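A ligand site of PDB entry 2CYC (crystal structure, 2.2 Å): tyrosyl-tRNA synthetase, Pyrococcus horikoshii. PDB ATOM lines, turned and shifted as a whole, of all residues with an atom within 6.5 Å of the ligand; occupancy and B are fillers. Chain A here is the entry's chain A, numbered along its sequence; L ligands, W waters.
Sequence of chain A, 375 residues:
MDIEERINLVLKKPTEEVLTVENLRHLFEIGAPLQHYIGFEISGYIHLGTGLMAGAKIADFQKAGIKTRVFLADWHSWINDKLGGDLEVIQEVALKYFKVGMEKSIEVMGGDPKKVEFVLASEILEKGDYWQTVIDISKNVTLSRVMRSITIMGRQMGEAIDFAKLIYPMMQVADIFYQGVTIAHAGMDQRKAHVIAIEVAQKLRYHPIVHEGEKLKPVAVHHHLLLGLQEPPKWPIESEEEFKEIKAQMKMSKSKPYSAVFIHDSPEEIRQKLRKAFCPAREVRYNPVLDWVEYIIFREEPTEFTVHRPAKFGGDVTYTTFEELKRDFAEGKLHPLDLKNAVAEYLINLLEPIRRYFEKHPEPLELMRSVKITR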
ATOM      1  N   TYR A  37      17.917  -6.510 -12.567  1.00  0.00           N
ATOM      2  CA  TYR A  37      19.191  -6.163 -12.009  1.00  0.00           C
ATOM      3  C   TYR A  37      19.651  -7.329 -11.142  1.00  0.00           C
ATOM      4  O   TYR A  37      18.854  -8.151 -10.689  1.00  0.00           O
ATOM      5  CB  TYR A  37      19.134  -4.871 -11.177  1.00  0.00           C
ATOM      6  CG  TYR A  37      19.223  -5.046  -9.668  1.00  0.00           C
ATOM      7  CD1 TYR A  37      20.212  -4.371  -8.925  1.00  0.00           C
ATOM      8  CD2 TYR A  37      18.290  -5.810  -8.967  1.00  0.00           C
ATOM      9  CE1 TYR A  37      20.246  -4.443  -7.523  1.00  0.00           C
ATOM     10  CE2 TYR A  37      18.316  -5.897  -7.566  1.00  0.00           C
ATOM     11  CZ  TYR A  37      19.291  -5.210  -6.855  1.00  0.00           C
ATOM     12  OH  TYR A  37      19.257  -5.231  -5.486  1.00  0.00           O
ATOM     13  N   ILE A  38      20.962  -7.394 -10.955  1.00  0.00           N
ATOM     14  CA  ILE A  38      21.577  -8.358 -10.068  1.00  0.00           C
ATOM     15  C   ILE A  38      22.836  -7.649  -9.604  1.00  0.00           C
ATOM     16  O   ILE A  38      23.630  -7.149 -10.421  1.00  0.00           O
ATOM     17  CB  ILE A  38      21.874  -9.760 -10.743  1.00  0.00           C
ATOM     18  CG1 ILE A  38      22.619 -10.644  -9.734  1.00  0.00           C
ATOM     19  CG2 ILE A  38      22.665  -9.611 -12.045  1.00  0.00           C
ATOM     20  CD1 ILE A  38      22.663 -12.127 -10.101  1.00  0.00           C
ATOM     21  N   GLY A  39      22.991  -7.541  -8.290  1.00  0.00           N
ATOM     22  CA  GLY A  39      24.136  -6.847  -7.736  1.00  0.00           C
ATOM     23  C   GLY A  39      25.228  -7.804  -7.296  1.00  0.00           C
ATOM     24  O   GLY A  39      24.974  -8.953  -6.943  1.00  0.00           O
ATOM     25  N   PHE A  40      26.463  -7.318  -7.314  1.00  0.00           N
ATOM     26  CA  PHE A  40      27.585  -8.148  -6.916  1.00  0.00           C
ATOM     27  C   PHE A  40      28.540  -7.340  -6.071  1.00  0.00           C
ATOM     28  O   PHE A  40      28.801  -6.163  -6.329  1.00  0.00           O
ATOM     29  CB  PHE A  40      28.390  -8.644  -8.111  1.00  0.00           C
ATOM     30  CG  PHE A  40      27.593  -9.382  -9.125  1.00  0.00           C
ATOM     31  CD1 PHE A  40      26.978  -8.705 -10.180  1.00  0.00           C
ATOM     32  CD2 PHE A  40      27.477 -10.769  -9.063  1.00  0.00           C
ATOM     33  CE1 PHE A  40      26.269  -9.392 -11.146  1.00  0.00           C
ATOM     34  CE2 PHE A  40      26.771 -11.463 -10.035  1.00  0.00           C
ATOM     35  CZ  PHE A  40      26.172 -10.778 -11.079  1.00  0.00           C
ATOM     36  N   GLU A  41      29.079  -7.981  -5.051  1.00  0.00           N
ATOM     37  CA  GLU A  41      30.086  -7.343  -4.244  1.00  0.00           C
ATOM     38  C   GLU A  41      31.341  -7.436  -5.117  1.00  0.00           C
ATOM     39  O   GLU A  41      31.428  -8.283  -6.001  1.00  0.00           O
ATOM     40  CB  GLU A  41      30.288  -8.092  -2.942  1.00  0.00           C
ATOM     41  CG  GLU A  41      29.264  -7.751  -1.858  1.00  0.00           C
ATOM     42  CD  GLU A  41      29.747  -8.137  -0.464  1.00  0.00           C
ATOM     43  OE1 GLU A  41      30.931  -8.526  -0.335  1.00  0.00           O
ATOM     44  OE2 GLU A  41      28.956  -8.045   0.499  1.00  0.00           O
ATOM     45  N   PHE A  71      24.712  -4.605 -11.407  1.00  0.00           N
ATOM     46  CA  PHE A  71      24.918  -3.597 -10.381  1.00  0.00           C
ATOM     47  C   PHE A  71      26.202  -3.924  -9.605  1.00  0.00           C
ATOM     48  O   PHE A  71      26.284  -4.948  -8.930  1.00  0.00           O
ATOM     49  CB  PHE A  71      23.699  -3.632  -9.442  1.00  0.00           C
ATOM     50  CG  PHE A  71      23.644  -2.520  -8.432  1.00  0.00           C
ATOM     51  CD1 PHE A  71      23.285  -1.225  -8.808  1.00  0.00           C
ATOM     52  CD2 PHE A  71      23.848  -2.790  -7.074  1.00  0.00           C
ATOM     53  CE1 PHE A  71      23.126  -0.222  -7.848  1.00  0.00           C
ATOM     54  CE2 PHE A  71      23.698  -1.793  -6.104  1.00  0.00           C
ATOM     55  CZ  PHE A  71      23.332  -0.499  -6.496  1.00  0.00           C
ATOM     56  N   ALA A  73      28.196  -3.323  -6.643  1.00  0.00           N
ATOM     57  CA  ALA A  73      27.990  -2.802  -5.284  1.00  0.00           C
ATOM     58  C   ALA A  73      29.249  -2.339  -4.568  1.00  0.00           C
ATOM     59  O   ALA A  73      29.704  -3.003  -3.625  1.00  0.00           O
ATOM     60  CB  ALA A  73      27.267  -3.878  -4.451  1.00  0.00           C
ATOM     61  N   HIS A  76      28.787  -1.089  -0.795  1.00  0.00           N
ATOM     62  CA  HIS A  76      28.390  -2.296  -0.080  1.00  0.00           C
ATOM     63  C   HIS A  76      29.624  -3.137   0.243  1.00  0.00           C
ATOM     64  O   HIS A  76      29.761  -3.641   1.349  1.00  0.00           O
ATOM     65  CB  HIS A  76      27.415  -3.146  -0.913  1.00  0.00           C
ATOM     66  CG  HIS A  76      26.206  -2.399  -1.401  1.00  0.00           C
ATOM     67  ND1 HIS A  76      26.283  -1.428  -2.384  1.00  0.00           N
ATOM     68  CD2 HIS A  76      24.896  -2.522  -1.091  1.00  0.00           C
ATOM     69  CE1 HIS A  76      25.065  -0.986  -2.648  1.00  0.00           C
ATOM     70  NE2 HIS A  76      24.202  -1.635  -1.884  1.00  0.00           N
ATOM     71  N   ASN A  80      31.319  -4.119   3.713  1.00  0.00           N
ATOM     72  CA  ASN A  80      31.576  -5.517   4.033  1.00  0.00           C
ATOM     73  C   ASN A  80      33.053  -5.885   4.093  1.00  0.00           C
ATOM     74  O   ASN A  80      33.407  -7.058   4.061  1.00  0.00           O
ATOM     75  CB  ASN A  80      30.825  -6.420   3.053  1.00  0.00           C
ATOM     76  CG  ASN A  80      30.472  -7.758   3.667  1.00  0.00           C
ATOM     77  OD1 ASN A  80      30.513  -7.904   4.893  1.00  0.00           O
ATOM     78  ND2 ASN A  80      30.113  -8.741   2.843  1.00  0.00           N
ATOM     79  N   ILE A 152      22.927 -12.463   4.052  1.00  0.00           N
ATOM     80  CA  ILE A 152      23.047 -12.178   2.625  1.00  0.00           C
ATOM     81  C   ILE A 152      24.436 -11.640   2.285  1.00  0.00           C
ATOM     82  O   ILE A 152      24.840 -11.670   1.109  1.00  0.00           O
ATOM     83  CB  ILE A 152      21.970 -11.162   2.105  1.00  0.00           C
ATOM     84  CG1 ILE A 152      22.157  -9.783   2.745  1.00  0.00           C
ATOM     85  CG2 ILE A 152      20.556 -11.699   2.375  1.00  0.00           C
ATOM     86  CD1 ILE A 152      21.139  -8.739   2.274  1.00  0.00           C
ATOM     87  N   MET A 153      25.174 -11.163   3.283  1.00  0.00           N
ATOM     88  CA  MET A 153      26.509 -10.659   3.011  1.00  0.00           C
ATOM     89  C   MET A 153      27.573 -11.622   3.482  1.00  0.00           C
ATOM     90  O   MET A 153      28.749 -11.265   3.623  1.00  0.00           O
ATOM     91  CB  MET A 153      26.704  -9.253   3.607  1.00  0.00           C
ATOM     92  CG  MET A 153      26.838  -9.143   5.098  1.00  0.00           C
ATOM     93  SD  MET A 153      26.712  -7.366   5.584  1.00  0.00           S
ATOM     94  CE  MET A 153      25.092  -7.310   5.883  1.00  0.00           C
ATOM     95  N   GLY A 154      27.154 -12.870   3.690  1.00  0.00           N
ATOM     96  CA  GLY A 154      28.053 -13.924   4.104  1.00  0.00           C
ATOM     97  C   GLY A 154      28.509 -13.847   5.549  1.00  0.00           C
ATOM     98  O   GLY A 154      29.560 -14.379   5.894  1.00  0.00           O
ATOM     99  N   TYR A 168      23.717  -2.179   5.394  1.00  0.00           N
ATOM    100  CA  TYR A 168      23.856  -2.905   4.124  1.00  0.00           C
ATOM    101  C   TYR A 168      22.570  -3.571   3.586  1.00  0.00           C
ATOM    102  O   TYR A 168      22.176  -3.349   2.439  1.00  0.00           O
ATOM    103  CB  TYR A 168      24.989  -3.941   4.280  1.00  0.00           C
ATOM    104  CG  TYR A 168      25.352  -4.785   3.062  1.00  0.00           C
ATOM    105  CD1 TYR A 168      26.681  -4.886   2.658  1.00  0.00           C
ATOM    106  CD2 TYR A 168      24.405  -5.545   2.384  1.00  0.00           C
ATOM    107  CE1 TYR A 168      27.064  -5.725   1.612  1.00  0.00           C
ATOM    108  CE2 TYR A 168      24.770  -6.400   1.334  1.00  0.00           C
ATOM    109  CZ  TYR A 168      26.112  -6.477   0.955  1.00  0.00           C
ATOM    110  OH  TYR A 168      26.501  -7.301  -0.076  1.00  0.00           O
ATOM    111  N   MET A 171      20.165  -1.108   2.297  1.00  0.00           N
ATOM    112  CA  MET A 171      20.645  -0.490   1.071  1.00  0.00           C
ATOM    113  C   MET A 171      20.315  -1.424  -0.113  1.00  0.00           C
ATOM    114  O   MET A 171      19.969  -0.946  -1.195  1.00  0.00           O
ATOM    115  CB  MET A 171      22.160  -0.281   1.133  1.00  0.00           C
ATOM    116  CG  MET A 171      22.600   0.868   2.042  1.00  0.00           C
ATOM    117  SD  MET A 171      24.388   0.797   2.344  1.00  0.00           S
ATOM    118  CE  MET A 171      25.035   1.062   0.659  1.00  0.00           C
ATOM    119  N   GLN A 172      20.425  -2.731   0.102  1.00  0.00           N
ATOM    120  CA  GLN A 172      20.131  -3.690  -0.962  1.00  0.00           C
ATOM    121  C   GLN A 172      18.671  -3.597  -1.354  1.00  0.00           C
ATOM    122  O   GLN A 172      18.328  -3.651  -2.541  1.00  0.00           O
ATOM    123  CB  GLN A 172      20.472  -5.133  -0.547  1.00  0.00           C
ATOM    124  CG  GLN A 172      20.297  -6.175  -1.695  1.00  0.00           C
ATOM    125  CD  GLN A 172      21.141  -7.426  -1.511  1.00  0.00           C
ATOM    126  OE1 GLN A 172      22.133  -7.412  -0.785  1.00  0.00           O
ATOM    127  NE2 GLN A 172      20.779  -8.514  -2.200  1.00  0.00           N
ATOM    128  N   VAL A 173      17.788  -3.460  -0.364  1.00  0.00           N
ATOM    129  CA  VAL A 173      16.369  -3.345  -0.675  1.00  0.00           C
ATOM    130  C   VAL A 173      16.101  -2.017  -1.402  1.00  0.00           C
ATOM    131  O   VAL A 173      15.367  -1.990  -2.402  1.00  0.00           O
ATOM    132  CB  VAL A 173      15.516  -3.443   0.610  1.00  0.00           C
ATOM    133  CG1 VAL A 173      14.069  -3.130   0.313  1.00  0.00           C
ATOM    134  CG2 VAL A 173      15.649  -4.845   1.192  1.00  0.00           C
ATOM    135  N   ASP A 175      18.143  -0.327  -3.215  1.00  0.00           N
ATOM    136  CA  ASP A 175      18.705  -0.407  -4.561  1.00  0.00           C
ATOM    137  C   ASP A 175      17.642  -0.889  -5.536  1.00  0.00           C
ATOM    138  O   ASP A 175      17.617  -0.467  -6.698  1.00  0.00           O
ATOM    139  CB  ASP A 175      19.875  -1.412  -4.616  1.00  0.00           C
ATOM    140  CG  ASP A 175      21.065  -0.969  -3.821  1.00  0.00           C
ATOM    141  OD1 ASP A 175      21.216   0.248  -3.583  1.00  0.00           O
ATOM    142  OD2 ASP A 175      21.867  -1.841  -3.447  1.00  0.00           O
ATOM    143  N   ILE A 176      16.782  -1.776  -5.058  1.00  0.00           N
ATOM    144  CA  ILE A 176      15.726  -2.306  -5.911  1.00  0.00           C
ATOM    145  C   ILE A 176      14.702  -1.249  -6.275  1.00  0.00           C
ATOM    146  O   ILE A 176      14.417  -1.008  -7.455  1.00  0.00           O
ATOM    147  CB  ILE A 176      15.015  -3.512  -5.222  1.00  0.00           C
ATOM    148  CG1 ILE A 176      15.958  -4.724  -5.205  1.00  0.00           C
ATOM    149  CG2 ILE A 176      13.708  -3.843  -5.949  1.00  0.00           C
ATOM    150  CD1 ILE A 176      15.498  -5.889  -4.326  1.00  0.00           C
ATOM    151  N   GLN A 179      15.969   2.000  -8.403  1.00  0.00           N
ATOM    152  CA  GLN A 179      16.190   1.773  -9.831  1.00  0.00           C
ATOM    153  C   GLN A 179      14.934   1.268 -10.545  1.00  0.00           C
ATOM    154  O   GLN A 179      14.971   0.960 -11.736  1.00  0.00           O
ATOM    155  CB  GLN A 179      17.325   0.750 -10.032  1.00  0.00           C
ATOM    156  CG  GLN A 179      18.629   1.103  -9.299  1.00  0.00           C
ATOM    157  CD  GLN A 179      19.698   0.035  -9.470  1.00  0.00           C
ATOM    158  OE1 GLN A 179      20.465   0.047 -10.451  1.00  0.00           O
ATOM    159  NE2 GLN A 179      19.760  -0.880  -8.522  1.00  0.00           N
ATOM    160  N   HIS A 185      16.879 -10.123  -9.464  1.00  0.00           N
ATOM    161  CA  HIS A 185      17.635 -11.348  -9.695  1.00  0.00           C
ATOM    162  C   HIS A 185      18.862 -11.499  -8.781  1.00  0.00           C
ATOM    163  O   HIS A 185      19.630 -10.546  -8.586  1.00  0.00           O
ATOM    164  CB  HIS A 185      18.039 -11.383 -11.176  1.00  0.00           C
ATOM    165  CG  HIS A 185      18.982 -12.478 -11.544  1.00  0.00           C
ATOM    166  ND1 HIS A 185      19.968 -12.323 -12.494  1.00  0.00           N
ATOM    167  CD2 HIS A 185      19.108 -13.739 -11.065  1.00  0.00           C
ATOM    168  CE1 HIS A 185      20.672 -13.436 -12.590  1.00  0.00           C
ATOM    169  NE2 HIS A 185      20.174 -14.313 -11.727  1.00  0.00           N
ATOM    170  N   ALA A 186      19.027 -12.696  -8.224  1.00  0.00           N
ATOM    171  CA  ALA A 186      20.160 -12.997  -7.340  1.00  0.00           C
ATOM    172  C   ALA A 186      20.291 -14.503  -7.154  1.00  0.00           C
ATOM    173  O   ALA A 186      19.448 -15.279  -7.609  1.00  0.00           O
ATOM    174  CB  ALA A 186      19.970 -12.332  -5.969  1.00  0.00           C
ATOM    175  N   ASP A 189      21.052 -17.346  -1.924  1.00  0.00           N
ATOM    176  CA  ASP A 189      21.446 -16.841  -0.616  1.00  0.00           C
ATOM    177  C   ASP A 189      21.089 -15.376  -0.359  1.00  0.00           C
ATOM    178  O   ASP A 189      21.304 -14.867   0.745  1.00  0.00           O
ATOM    179  CB  ASP A 189      22.949 -17.074  -0.360  1.00  0.00           C
ATOM    180  CG  ASP A 189      23.856 -16.514  -1.458  1.00  0.00           C
ATOM    181  OD1 ASP A 189      23.379 -15.806  -2.365  1.00  0.00           O
ATOM    182  OD2 ASP A 189      25.071 -16.785  -1.408  1.00  0.00           O
ATOM    183  N   GLN A 190      20.544 -14.714  -1.360  1.00  0.00           N
ATOM    184  CA  GLN A 190      20.146 -13.316  -1.212  1.00  0.00           C
ATOM    185  C   GLN A 190      18.632 -13.205  -1.035  1.00  0.00           C
ATOM    186  O   GLN A 190      18.131 -12.096  -0.882  1.00  0.00           O
ATOM    187  CB  GLN A 190      20.524 -12.521  -2.456  1.00  0.00           C
ATOM    188  CG  GLN A 190      22.004 -12.582  -2.811  1.00  0.00           C
ATOM    189  CD  GLN A 190      22.853 -12.075  -1.685  1.00  0.00           C
ATOM    190  OE1 GLN A 190      22.739 -10.926  -1.267  1.00  0.00           O
ATOM    191  NE2 GLN A 190      23.726 -12.948  -1.178  1.00  0.00           N
ATOM    192  N   HIS A 194      15.045 -10.031  -0.736  1.00  0.00           N
ATOM    193  CA  HIS A 194      13.942  -9.945  -1.675  1.00  0.00           C
ATOM    194  C   HIS A 194      12.599 -10.187  -0.974  1.00  0.00           C
ATOM    195  O   HIS A 194      11.581  -9.591  -1.349  1.00  0.00           O
ATOM    196  CB  HIS A 194      14.196 -10.912  -2.833  1.00  0.00           C
ATOM    197  CG  HIS A 194      15.358 -10.499  -3.695  1.00  0.00           C
ATOM    198  ND1 HIS A 194      15.881 -11.298  -4.695  1.00  0.00           N
ATOM    199  CD2 HIS A 194      16.064  -9.338  -3.743  1.00  0.00           C
ATOM    200  CE1 HIS A 194      16.854 -10.654  -5.309  1.00  0.00           C
ATOM    201  NE2 HIS A 194      16.983  -9.460  -4.754  1.00  0.00           N
HETATM  202  N1  LIG L   1      24.571  -8.891  -1.255  1.00  0.00           N
HETATM  203  C1  LIG L   1      25.046  -9.283  -2.614  1.00  0.00           C
HETATM  204  C2  LIG L   1      26.145 -10.339  -2.524  1.00  0.00           C
HETATM  205  O1  LIG L   1      26.618 -10.593  -1.393  1.00  0.00           O
HETATM  206  C3  LIG L   1      25.563  -8.050  -3.366  1.00  0.00           C
HETATM  207  C4  LIG L   1      24.490  -7.012  -3.646  1.00  0.00           C
HETATM  208  C5  LIG L   1      23.369  -7.328  -4.424  1.00  0.00           C
HETATM  209  C6  LIG L   1      24.588  -5.716  -3.126  1.00  0.00           C
HETATM  210  C7  LIG L   1      22.378  -6.368  -4.681  1.00  0.00           C
HETATM  211  C8  LIG L   1      23.606  -4.762  -3.373  1.00  0.00           C
HETATM  212  C9  LIG L   1      22.505  -5.091  -4.145  1.00  0.00           C
HETATM  213  O2  LIG L   1      21.529  -4.135  -4.376  1.00  0.00           O
HETATM  214  O3  LIG L   1      26.528 -10.887  -3.577  1.00  0.00           O
HETATM  215  O   HOH W   1      28.947 -11.335  -4.772  1.00  0.00           O
HETATM  216  O   HOH W   2      26.763 -13.515  -2.815  1.00  0.00           O
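O of Ile 152 lies close to O1 of the ligand (3.3 Å). Merely in contact with the ligand: Gly 39, Glu 41, Phe 71, Ala 73 and His 76. Hydrophobic or aromatic side chains that line the ligand: Tyr 37, Phe 71, Ala 73, His 76 and Tyr 168. Of the 24 residues printed, 11 come within 4 Å of the ligand. The nearest printed residue that does not touch the ligand is Phe 40 (4.1 Å).
The side-chain hydroxyl (OH) of Tyr 37 is in hydrogen-bond range of an oxygen (O2) of the ligand. OH of Tyr 168 sits at hydrogen-bond distance from N1 of the ligand. OD2 of Asp 175 sits at hydrogen-bond distance from O2 of the ligand, 2.5 Å away. OE1 of Gln 190 sits at hydrogen-bond distance from N1 of the ligand (2.7 Å). A nitrogen (N1) of the ligand sits at hydrogen-bond distance from the side-chain amide oxygen of Gln 172 (2.9 Å).
O of Ile 152 is in hydrogen-bond range of NE2 of Gln 190 (2.8 Å). N of Ala 73 lies within hydrogen-bond range of O of Phe 40 (2.9 Å). The side-chain carboxylate (OE2) of Glu 41 lies within hydrogen-bond range of the side-chain amide nitrogen (ND2) of Asn 80 (2.7 Å). The side-chain hydroxyl (OH) of Tyr 168 lies within hydrogen-bond range of the side-chain carboxylate (OE2) of Glu 41, 2.6 Å away. The side-chain amide nitrogen of Gln 179 sits at hydrogen-bond distance from the backbone carbonyl oxygen of Asp 175. O of Ile 38 lies within hydrogen-bond range of N of Phe 71, 2.9 Å away. OH of Tyr 37 is in hydrogen-bond range of O of Gln 172. OE1 of Gln 190 is in hydrogen-bond range of NE2 of Gln 172, at 3.2 Å.
Water W1 lies within hydrogen-bond range of an oxygen (O3) of the ligand (2.7 Å) and the backbone NH of Glu 41 (3.4 Å). Water W2 lies within hydrogen-bond range of O3 of the ligand (2.7 Å) and NE2 of Gln 190 (3.5 Å).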
